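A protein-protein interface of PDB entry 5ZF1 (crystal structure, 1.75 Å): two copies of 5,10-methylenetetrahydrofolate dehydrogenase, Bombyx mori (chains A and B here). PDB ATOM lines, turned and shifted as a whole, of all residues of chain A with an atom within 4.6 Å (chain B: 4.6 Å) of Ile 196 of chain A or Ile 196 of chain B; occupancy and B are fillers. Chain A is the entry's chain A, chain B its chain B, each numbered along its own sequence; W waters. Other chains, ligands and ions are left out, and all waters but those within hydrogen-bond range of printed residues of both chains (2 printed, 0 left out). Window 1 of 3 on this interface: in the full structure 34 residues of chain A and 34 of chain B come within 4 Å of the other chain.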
ATOM      1  N   VAL A 163      18.112 -12.563 -22.363  1.00  0.00           N
ATOM      2  CA  VAL A 163      19.396 -12.048 -22.817  1.00  0.00           C
ATOM      3  C   VAL A 163      19.824 -12.964 -23.947  1.00  0.00           C
ATOM      4  O   VAL A 163      19.905 -14.181 -23.752  1.00  0.00           O
ATOM      5  CB  VAL A 163      20.446 -12.031 -21.698  1.00  0.00           C
ATOM      6  CG1 VAL A 163      21.829 -11.648 -22.243  1.00  0.00           C
ATOM      7  CG2 VAL A 163      20.006 -11.058 -20.555  1.00  0.00           C
ATOM      8  N   GLY A 165      22.796 -14.062 -26.332  1.00  0.00           N
ATOM      9  CA  GLY A 165      24.239 -13.962 -26.329  1.00  0.00           C
ATOM     10  C   GLY A 165      24.868 -14.318 -25.003  1.00  0.00           C
ATOM     11  O   GLY A 165      24.391 -13.890 -23.941  1.00  0.00           O
ATOM     12  N   ARG A 166      25.928 -15.121 -25.051  1.00  0.00           N
ATOM     13  CA  ARG A 166      26.658 -15.578 -23.878  1.00  0.00           C
ATOM     14  C   ARG A 166      28.048 -14.980 -23.770  1.00  0.00           C
ATOM     15  O   ARG A 166      28.862 -15.496 -23.002  1.00  0.00           O
ATOM     16  CB  ARG A 166      26.831 -17.097 -23.910  1.00  0.00           C
ATOM     17  CG  ARG A 166      25.603 -17.922 -23.865  1.00  0.00           C
ATOM     18  CD  ARG A 166      25.997 -19.390 -24.085  1.00  0.00           C
ATOM     19  NE  ARG A 166      26.355 -19.697 -25.474  1.00  0.00           N
ATOM     20  CZ  ARG A 166      26.475 -20.939 -25.946  1.00  0.00           C
ATOM     21  NH1 ARG A 166      26.283 -21.973 -25.131  1.00  0.00           N
ATOM     22  NH2 ARG A 166      26.785 -21.160 -27.215  1.00  0.00           N
ATOM     23  N   ALA A 175      23.519 -10.844 -18.125  1.00  0.00           N
ATOM     24  CA  ALA A 175      22.602 -11.804 -17.542  1.00  0.00           C
ATOM     25  C   ALA A 175      22.880 -12.001 -16.060  1.00  0.00           C
ATOM     26  O   ALA A 175      21.943 -12.229 -15.279  1.00  0.00           O
ATOM     27  CB  ALA A 175      22.684 -13.137 -18.295  1.00  0.00           C
ATOM     28  N   HIS A 179      19.692 -10.962 -13.237  1.00  0.00           N
ATOM     29  CA  HIS A 179      18.947 -11.921 -12.424  1.00  0.00           C
ATOM     30  C   HIS A 179      19.289 -11.886 -10.939  1.00  0.00           C
ATOM     31  O   HIS A 179      18.589 -12.540 -10.152  1.00  0.00           O
ATOM     32  CB  HIS A 179      19.166 -13.363 -12.949  1.00  0.00           C
ATOM     33  CG  HIS A 179      20.367 -14.049 -12.375  1.00  0.00           C
ATOM     34  ND1 HIS A 179      21.590 -14.057 -13.010  1.00  0.00           N
ATOM     35  CD2 HIS A 179      20.533 -14.758 -11.231  1.00  0.00           C
ATOM     36  CE1 HIS A 179      22.466 -14.727 -12.279  1.00  0.00           C
ATOM     37  NE2 HIS A 179      21.848 -15.170 -11.195  1.00  0.00           N
ATOM     38  N   THR A 193      13.764 -12.419 -13.661  1.00  0.00           N
ATOM     39  CA  THR A 193      13.872 -13.798 -14.136  1.00  0.00           C
ATOM     40  C   THR A 193      14.507 -13.753 -15.511  1.00  0.00           C
ATOM     41  O   THR A 193      14.020 -13.023 -16.374  1.00  0.00           O
ATOM     42  CB  THR A 193      12.484 -14.417 -14.234  1.00  0.00           C
ATOM     43  OG1 THR A 193      11.853 -14.356 -12.957  1.00  0.00           O
ATOM     44  CG2 THR A 193      12.573 -15.871 -14.651  1.00  0.00           C
ATOM     45  N   VAL A 194      15.584 -14.514 -15.728  1.00  0.00           N
ATOM     46  CA  VAL A 194      16.400 -14.323 -16.924  1.00  0.00           C
ATOM     47  C   VAL A 194      16.528 -15.627 -17.694  1.00  0.00           C
ATOM     48  O   VAL A 194      16.953 -16.638 -17.136  1.00  0.00           O
ATOM     49  CB  VAL A 194      17.799 -13.786 -16.588  1.00  0.00           C
ATOM     50  CG1 VAL A 194      18.623 -13.652 -17.859  1.00  0.00           C
ATOM     51  CG2 VAL A 194      17.643 -12.402 -15.953  1.00  0.00           C
ATOM     52  N   THR A 195      16.181 -15.585 -18.969  1.00  0.00           N
ATOM     53  CA  THR A 195      16.480 -16.685 -19.883  1.00  0.00           C
ATOM     54  C   THR A 195      17.640 -16.264 -20.763  1.00  0.00           C
ATOM     55  O   THR A 195      17.594 -15.195 -21.380  1.00  0.00           O
ATOM     56  CB  THR A 195      15.274 -17.024 -20.756  1.00  0.00           C
ATOM     57  OG1 THR A 195      14.156 -17.357 -19.937  1.00  0.00           O
ATOM     58  CG2 THR A 195      15.626 -18.210 -21.706  1.00  0.00           C
ATOM     59  N   ILE A 196      18.643 -17.139 -20.876  1.00  0.00           N
ATOM     60  CA  ILE A 196      19.815 -16.903 -21.702  1.00  0.00           C
ATOM     61  C   ILE A 196      19.642 -17.726 -22.974  1.00  0.00           C
ATOM     62  O   ILE A 196      19.663 -18.959 -22.921  1.00  0.00           O
ATOM     63  CB  ILE A 196      21.105 -17.291 -20.970  1.00  0.00           C
ATOM     64  CG1 ILE A 196      21.317 -16.357 -19.769  1.00  0.00           C
ATOM     65  CG2 ILE A 196      22.312 -17.239 -21.931  1.00  0.00           C
ATOM     66  CD1 ILE A 196      21.232 -17.063 -18.453  1.00  0.00           C
ATOM     67  N   CYS A 197      19.463 -17.046 -24.094  1.00  0.00           N
ATOM     68  CA  CYS A 197      19.377 -17.691 -25.404  1.00  0.00           C
ATOM     69  C   CYS A 197      20.678 -17.458 -26.145  1.00  0.00           C
ATOM     70  O   CYS A 197      21.390 -16.493 -25.883  1.00  0.00           O
ATOM     71  CB  CYS A 197      18.209 -17.147 -26.219  1.00  0.00           C
ATOM     72  SG  CYS A 197      16.593 -17.443 -25.464  1.00  0.00           S
ATOM     73  N   HIS A 198      21.006 -18.364 -27.067  1.00  0.00           N
ATOM     74  CA  HIS A 198      22.317 -18.278 -27.703  1.00  0.00           C
ATOM     75  C   HIS A 198      22.224 -18.957 -29.064  1.00  0.00           C
ATOM     76  O   HIS A 198      21.129 -19.241 -29.554  1.00  0.00           O
ATOM     77  CB  HIS A 198      23.406 -18.909 -26.824  1.00  0.00           C
ATOM     78  CG  HIS A 198      23.062 -20.278 -26.322  1.00  0.00           C
ATOM     79  ND1 HIS A 198      23.039 -21.385 -27.147  1.00  0.00           N
ATOM     80  CD2 HIS A 198      22.728 -20.719 -25.087  1.00  0.00           C
ATOM     81  CE1 HIS A 198      22.706 -22.452 -26.437  1.00  0.00           C
ATOM     82  NE2 HIS A 198      22.524 -22.078 -25.181  1.00  0.00           N
ATOM     83  N   VAL B 163      16.412 -23.505 -13.940  1.00  0.00           N
ATOM     84  CA  VAL B 163      17.093 -23.708 -12.668  1.00  0.00           C
ATOM     85  C   VAL B 163      16.358 -22.836 -11.668  1.00  0.00           C
ATOM     86  O   VAL B 163      16.290 -21.618 -11.863  1.00  0.00           O
ATOM     87  CB  VAL B 163      18.573 -23.312 -12.736  1.00  0.00           C
ATOM     88  CG1 VAL B 163      19.226 -23.526 -11.362  1.00  0.00           C
ATOM     89  CG2 VAL B 163      19.321 -24.121 -13.826  1.00  0.00           C
ATOM     90  N   GLY B 165      16.582 -21.302  -8.277  1.00  0.00           N
ATOM     91  CA  GLY B 165      17.612 -21.035  -7.280  1.00  0.00           C
ATOM     92  C   GLY B 165      18.792 -20.380  -7.960  1.00  0.00           C
ATOM     93  O   GLY B 165      19.258 -20.810  -9.013  1.00  0.00           O
ATOM     94  N   ARG B 166      19.277 -19.282  -7.361  1.00  0.00           N
ATOM     95  CA  ARG B 166      20.388 -18.496  -7.896  1.00  0.00           C
ATOM     96  C   ARG B 166      21.560 -18.395  -6.921  1.00  0.00           C
ATOM     97  O   ARG B 166      22.413 -17.502  -7.072  1.00  0.00           O
ATOM     98  CB  ARG B 166      19.915 -17.089  -8.288  1.00  0.00           C
ATOM     99  CG  ARG B 166      19.357 -16.291  -7.104  1.00  0.00           C
ATOM    100  CD  ARG B 166      18.867 -14.913  -7.524  1.00  0.00           C
ATOM    101  NE  ARG B 166      18.218 -14.291  -6.360  1.00  0.00           N
ATOM    102  CZ  ARG B 166      17.619 -13.104  -6.367  1.00  0.00           C
ATOM    103  NH1 ARG B 166      17.588 -12.367  -7.469  1.00  0.00           N
ATOM    104  NH2 ARG B 166      17.051 -12.663  -5.254  1.00  0.00           N
ATOM    105  N   ALA B 175      23.464 -23.183 -13.337  1.00  0.00           N
ATOM    106  CA  ALA B 175      22.999 -22.486 -14.537  1.00  0.00           C
ATOM    107  C   ALA B 175      24.147 -22.178 -15.481  1.00  0.00           C
ATOM    108  O   ALA B 175      24.002 -22.305 -16.705  1.00  0.00           O
ATOM    109  CB  ALA B 175      22.272 -21.193 -14.152  1.00  0.00           C
ATOM    110  N   HIS B 179      24.477 -23.786 -19.562  1.00  0.00           N
ATOM    111  CA  HIS B 179      24.554 -23.023 -20.801  1.00  0.00           C
ATOM    112  C   HIS B 179      26.001 -22.862 -21.275  1.00  0.00           C
ATOM    113  O   HIS B 179      26.298 -21.978 -22.073  1.00  0.00           O
ATOM    114  CB  HIS B 179      23.813 -21.681 -20.683  1.00  0.00           C
ATOM    115  CG  HIS B 179      24.443 -20.655 -19.779  1.00  0.00           C
ATOM    116  ND1 HIS B 179      25.560 -19.932 -20.130  1.00  0.00           N
ATOM    117  CD2 HIS B 179      24.041 -20.159 -18.581  1.00  0.00           C
ATOM    118  CE1 HIS B 179      25.861 -19.082 -19.162  1.00  0.00           C
ATOM    119  NE2 HIS B 179      24.950 -19.200 -18.210  1.00  0.00           N
ATOM    120  N   THR B 193      19.340 -23.914 -23.213  1.00  0.00           N
ATOM    121  CA  THR B 193      18.731 -22.592 -23.055  1.00  0.00           C
ATOM    122  C   THR B 193      18.212 -22.522 -21.619  1.00  0.00           C
ATOM    123  O   THR B 193      17.272 -23.227 -21.276  1.00  0.00           O
ATOM    124  CB  THR B 193      17.583 -22.415 -24.048  1.00  0.00           C
ATOM    125  OG1 THR B 193      18.067 -22.607 -25.384  1.00  0.00           O
ATOM    126  CG2 THR B 193      16.970 -21.003 -23.927  1.00  0.00           C
ATOM    127  N   VAL B 194      18.794 -21.660 -20.783  1.00  0.00           N
ATOM    128  CA  VAL B 194      18.603 -21.752 -19.332  1.00  0.00           C
ATOM    129  C   VAL B 194      17.789 -20.561 -18.869  1.00  0.00           C
ATOM    130  O   VAL B 194      18.106 -19.427 -19.228  1.00  0.00           O
ATOM    131  CB  VAL B 194      19.950 -21.778 -18.591  1.00  0.00           C
ATOM    132  CG1 VAL B 194      19.741 -21.774 -17.088  1.00  0.00           C
ATOM    133  CG2 VAL B 194      20.756 -23.011 -18.974  1.00  0.00           C
ATOM    134  N   THR B 195      16.748 -20.815 -18.078  1.00  0.00           N
ATOM    135  CA  THR B 195      16.042 -19.748 -17.367  1.00  0.00           C
ATOM    136  C   THR B 195      16.409 -19.864 -15.904  1.00  0.00           C
ATOM    137  O   THR B 195      16.326 -20.953 -15.334  1.00  0.00           O
ATOM    138  CB  THR B 195      14.527 -19.884 -17.522  1.00  0.00           C
ATOM    139  OG1 THR B 195      14.181 -19.870 -18.911  1.00  0.00           O
ATOM    140  CG2 THR B 195      13.804 -18.733 -16.759  1.00  0.00           C
ATOM    141  N   ILE B 196      16.824 -18.750 -15.299  1.00  0.00           N
ATOM    142  CA  ILE B 196      17.135 -18.686 -13.880  1.00  0.00           C
ATOM    143  C   ILE B 196      15.906 -18.107 -13.198  1.00  0.00           C
ATOM    144  O   ILE B 196      15.565 -16.945 -13.427  1.00  0.00           O
ATOM    145  CB  ILE B 196      18.357 -17.800 -13.613  1.00  0.00           C
ATOM    146  CG1 ILE B 196      19.598 -18.386 -14.316  1.00  0.00           C
ATOM    147  CG2 ILE B 196      18.611 -17.700 -12.128  1.00  0.00           C
ATOM    148  CD1 ILE B 196      20.673 -17.345 -14.547  1.00  0.00           C
ATOM    149  N   CYS B 197      15.232 -18.932 -12.409  1.00  0.00           N
ATOM    150  CA  CYS B 197      14.141 -18.493 -11.552  1.00  0.00           C
ATOM    151  C   CYS B 197      14.652 -18.430 -10.124  1.00  0.00           C
ATOM    152  O   CYS B 197      15.638 -19.077  -9.768  1.00  0.00           O
ATOM    153  CB  CYS B 197      12.948 -19.447 -11.646  1.00  0.00           C
ATOM    154  SG  CYS B 197      12.151 -19.497 -13.271  1.00  0.00           S
ATOM    155  N   HIS B 198      13.974 -17.636  -9.298  1.00  0.00           N
ATOM    156  CA  HIS B 198      14.496 -17.402  -7.953  1.00  0.00           C
ATOM    157  C   HIS B 198      13.365 -16.924  -7.052  1.00  0.00           C
ATOM    158  O   HIS B 198      12.188 -16.962  -7.423  1.00  0.00           O
ATOM    159  CB  HIS B 198      15.649 -16.392  -7.961  1.00  0.00           C
ATOM    160  CG  HIS B 198      15.340 -15.118  -8.688  1.00  0.00           C
ATOM    161  ND1 HIS B 198      14.439 -14.178  -8.217  1.00  0.00           N
ATOM    162  CD2 HIS B 198      15.824 -14.625  -9.855  1.00  0.00           C
ATOM    163  CE1 HIS B 198      14.384 -13.165  -9.068  1.00  0.00           C
ATOM    164  NE2 HIS B 198      15.204 -13.420 -10.077  1.00  0.00           N
HETATM  165  O   HOH W   1      21.380 -20.608 -21.840  1.00  0.00           O
HETATM  166  O   HOH W   2      23.133 -15.425  -8.617  1.00  0.00           O
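NH1 of Arg 166 of chain A lies within hydrogen-bond range of O of His 179 of chain B.
The backbone NH of Ile 196 of chain B is in hydrogen-bond range of the backbone carbonyl oxygen of Val 194 of chain A (2.8 Å).
The backbone carbonyl oxygen (O) of His 179 of chain A sits close to a ring nitrogen (NE2) of His 198 of chain B, 3.5 Å away.
The backbone carbonyl oxygen of His 179 of chain A lies within hydrogen-bond range of the guanidinium group of Arg 166 of chain B (2.9 Å).
N of Ile 196 of chain A sits at hydrogen-bond distance from O of Val 194 of chain B (2.9 Å).
The side-chain hydroxyl of Thr 195 of chain A lies within hydrogen-bond range of the side-chain hydroxyl of Thr 195 of chain B, 2.7 Å away.
N of Gly 165 of chain A lies within hydrogen-bond range of O of Cys 197 of chain A.
The backbone carbonyl oxygen of Ala 175 of chain A lies within hydrogen-bond range of a ring nitrogen (ND1) of His 179 of chain A.
N of Val 163 of chain B sits at hydrogen-bond distance from O of Thr 195 of chain B (2.9 Å).
The backbone NH of Cys 197 of chain A lies within hydrogen-bond range of the backbone carbonyl oxygen of Val 163 of chain A, at 2.9 Å.
The backbone NH of Gly 165 of chain B is in hydrogen-bond range of the backbone carbonyl oxygen of Cys 197 of chain B (2.8 Å).
O of Thr 195 of chain A sits at hydrogen-bond distance from N of Val 163 of chain A, 2.9 Å away.
Among the printed residues, pairs that only touch across the chains: Val 194 of chain A with Thr 195 of chain B (3.2 Å), Thr 195 of chain A with Val 194 of chain B (3.3 Å), Thr 193 of chain A with Ile 196 of chain B (3.4 Å), Ile 196 of chain A with Thr 193 of chain B (3.5 Å), His 179 of chain A with Ile 196 of chain B (3.6 Å), Val 194 of chain A with Val 194 of chain B (3.7 Å), Thr 193 of chain A with Thr 195 of chain B (3.8 Å), Thr 195 of chain A with Thr 193 of chain B (3.8 Å), Cys 197 of chain A with Thr 193 of chain B (3.9 Å), Thr 193 of chain A with Cys 197 of chain B (3.9 Å), Ile 196 of chain A with Ile 196 of chain B (3.96 Å) and Thr 193 of chain A with His 198 of chain B (3.99 Å).
Ile 196 of chain A touches just these residues of chain B: Thr 193, Val 194 and Ile 196.
Ile 196 of chain B touches four residues of chain A.
Of the printed residues of chain A, His 179 of chain B touches Arg 166.
Printed residues of chain B within 4 Å of Thr 195 of chain A: Thr 193 (3.8 Å), Val 194 (3.3 Å) and Thr 195 (2.7 Å).
Of the printed residues of chain B, Val 194 of chain A touches Val 194, Thr 195 and Ile 196.
Gly 165 of chain A touches none of the printed residues of chain B.
Val 163 of chain B touches none of the printed residues of chain A.
The nearest residue of chain B that does not touch Ile 196 of chain A is His 179 of chain B (4.2 Å).
Of the 11 printed residues of chain B, 8 touch a printed residue of chain A.
Hydrophobic or aromatic side chains of chain B within 4 Å of the printed part of chain A: Ile 196 and His 198.
Hydrophobic or aromatic side chains of chain A within 4 Å of the printed part of chain B: His 179 and Ile 196.
Among the printed residues, 18 pairs touch across the chains.
Among the printed residues, no Asp or Glu carboxylate lies within 4 Å of a Lys or Arg side-chain nitrogen of the other chain.
Thr 193 of chain A touches Cys 197 of chain B, and with the chains exchanged Cys 197 of chain A touches Thr 193 of chain B.
Val 194 of chain A touches its own counterpart, Val 194 of chain B.
Thr 195 of chain B touches its own counterpart, Thr 195 of chain A.
Ile 196 of chain A touches its own counterpart, Ile 196 of chain B.
11 positions are printed for both chains.
Water W1 bridges O of Ile 196 of chain A (2.6 Å) and N of Val 194 of chain B (3.0 Å).
Water W2 lies within hydrogen-bond range of the backbone carbonyl oxygen of Arg 166 of chain B (2.7 Å) and a ring nitrogen (NE2) of His 179 of chain A (2.9 Å).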
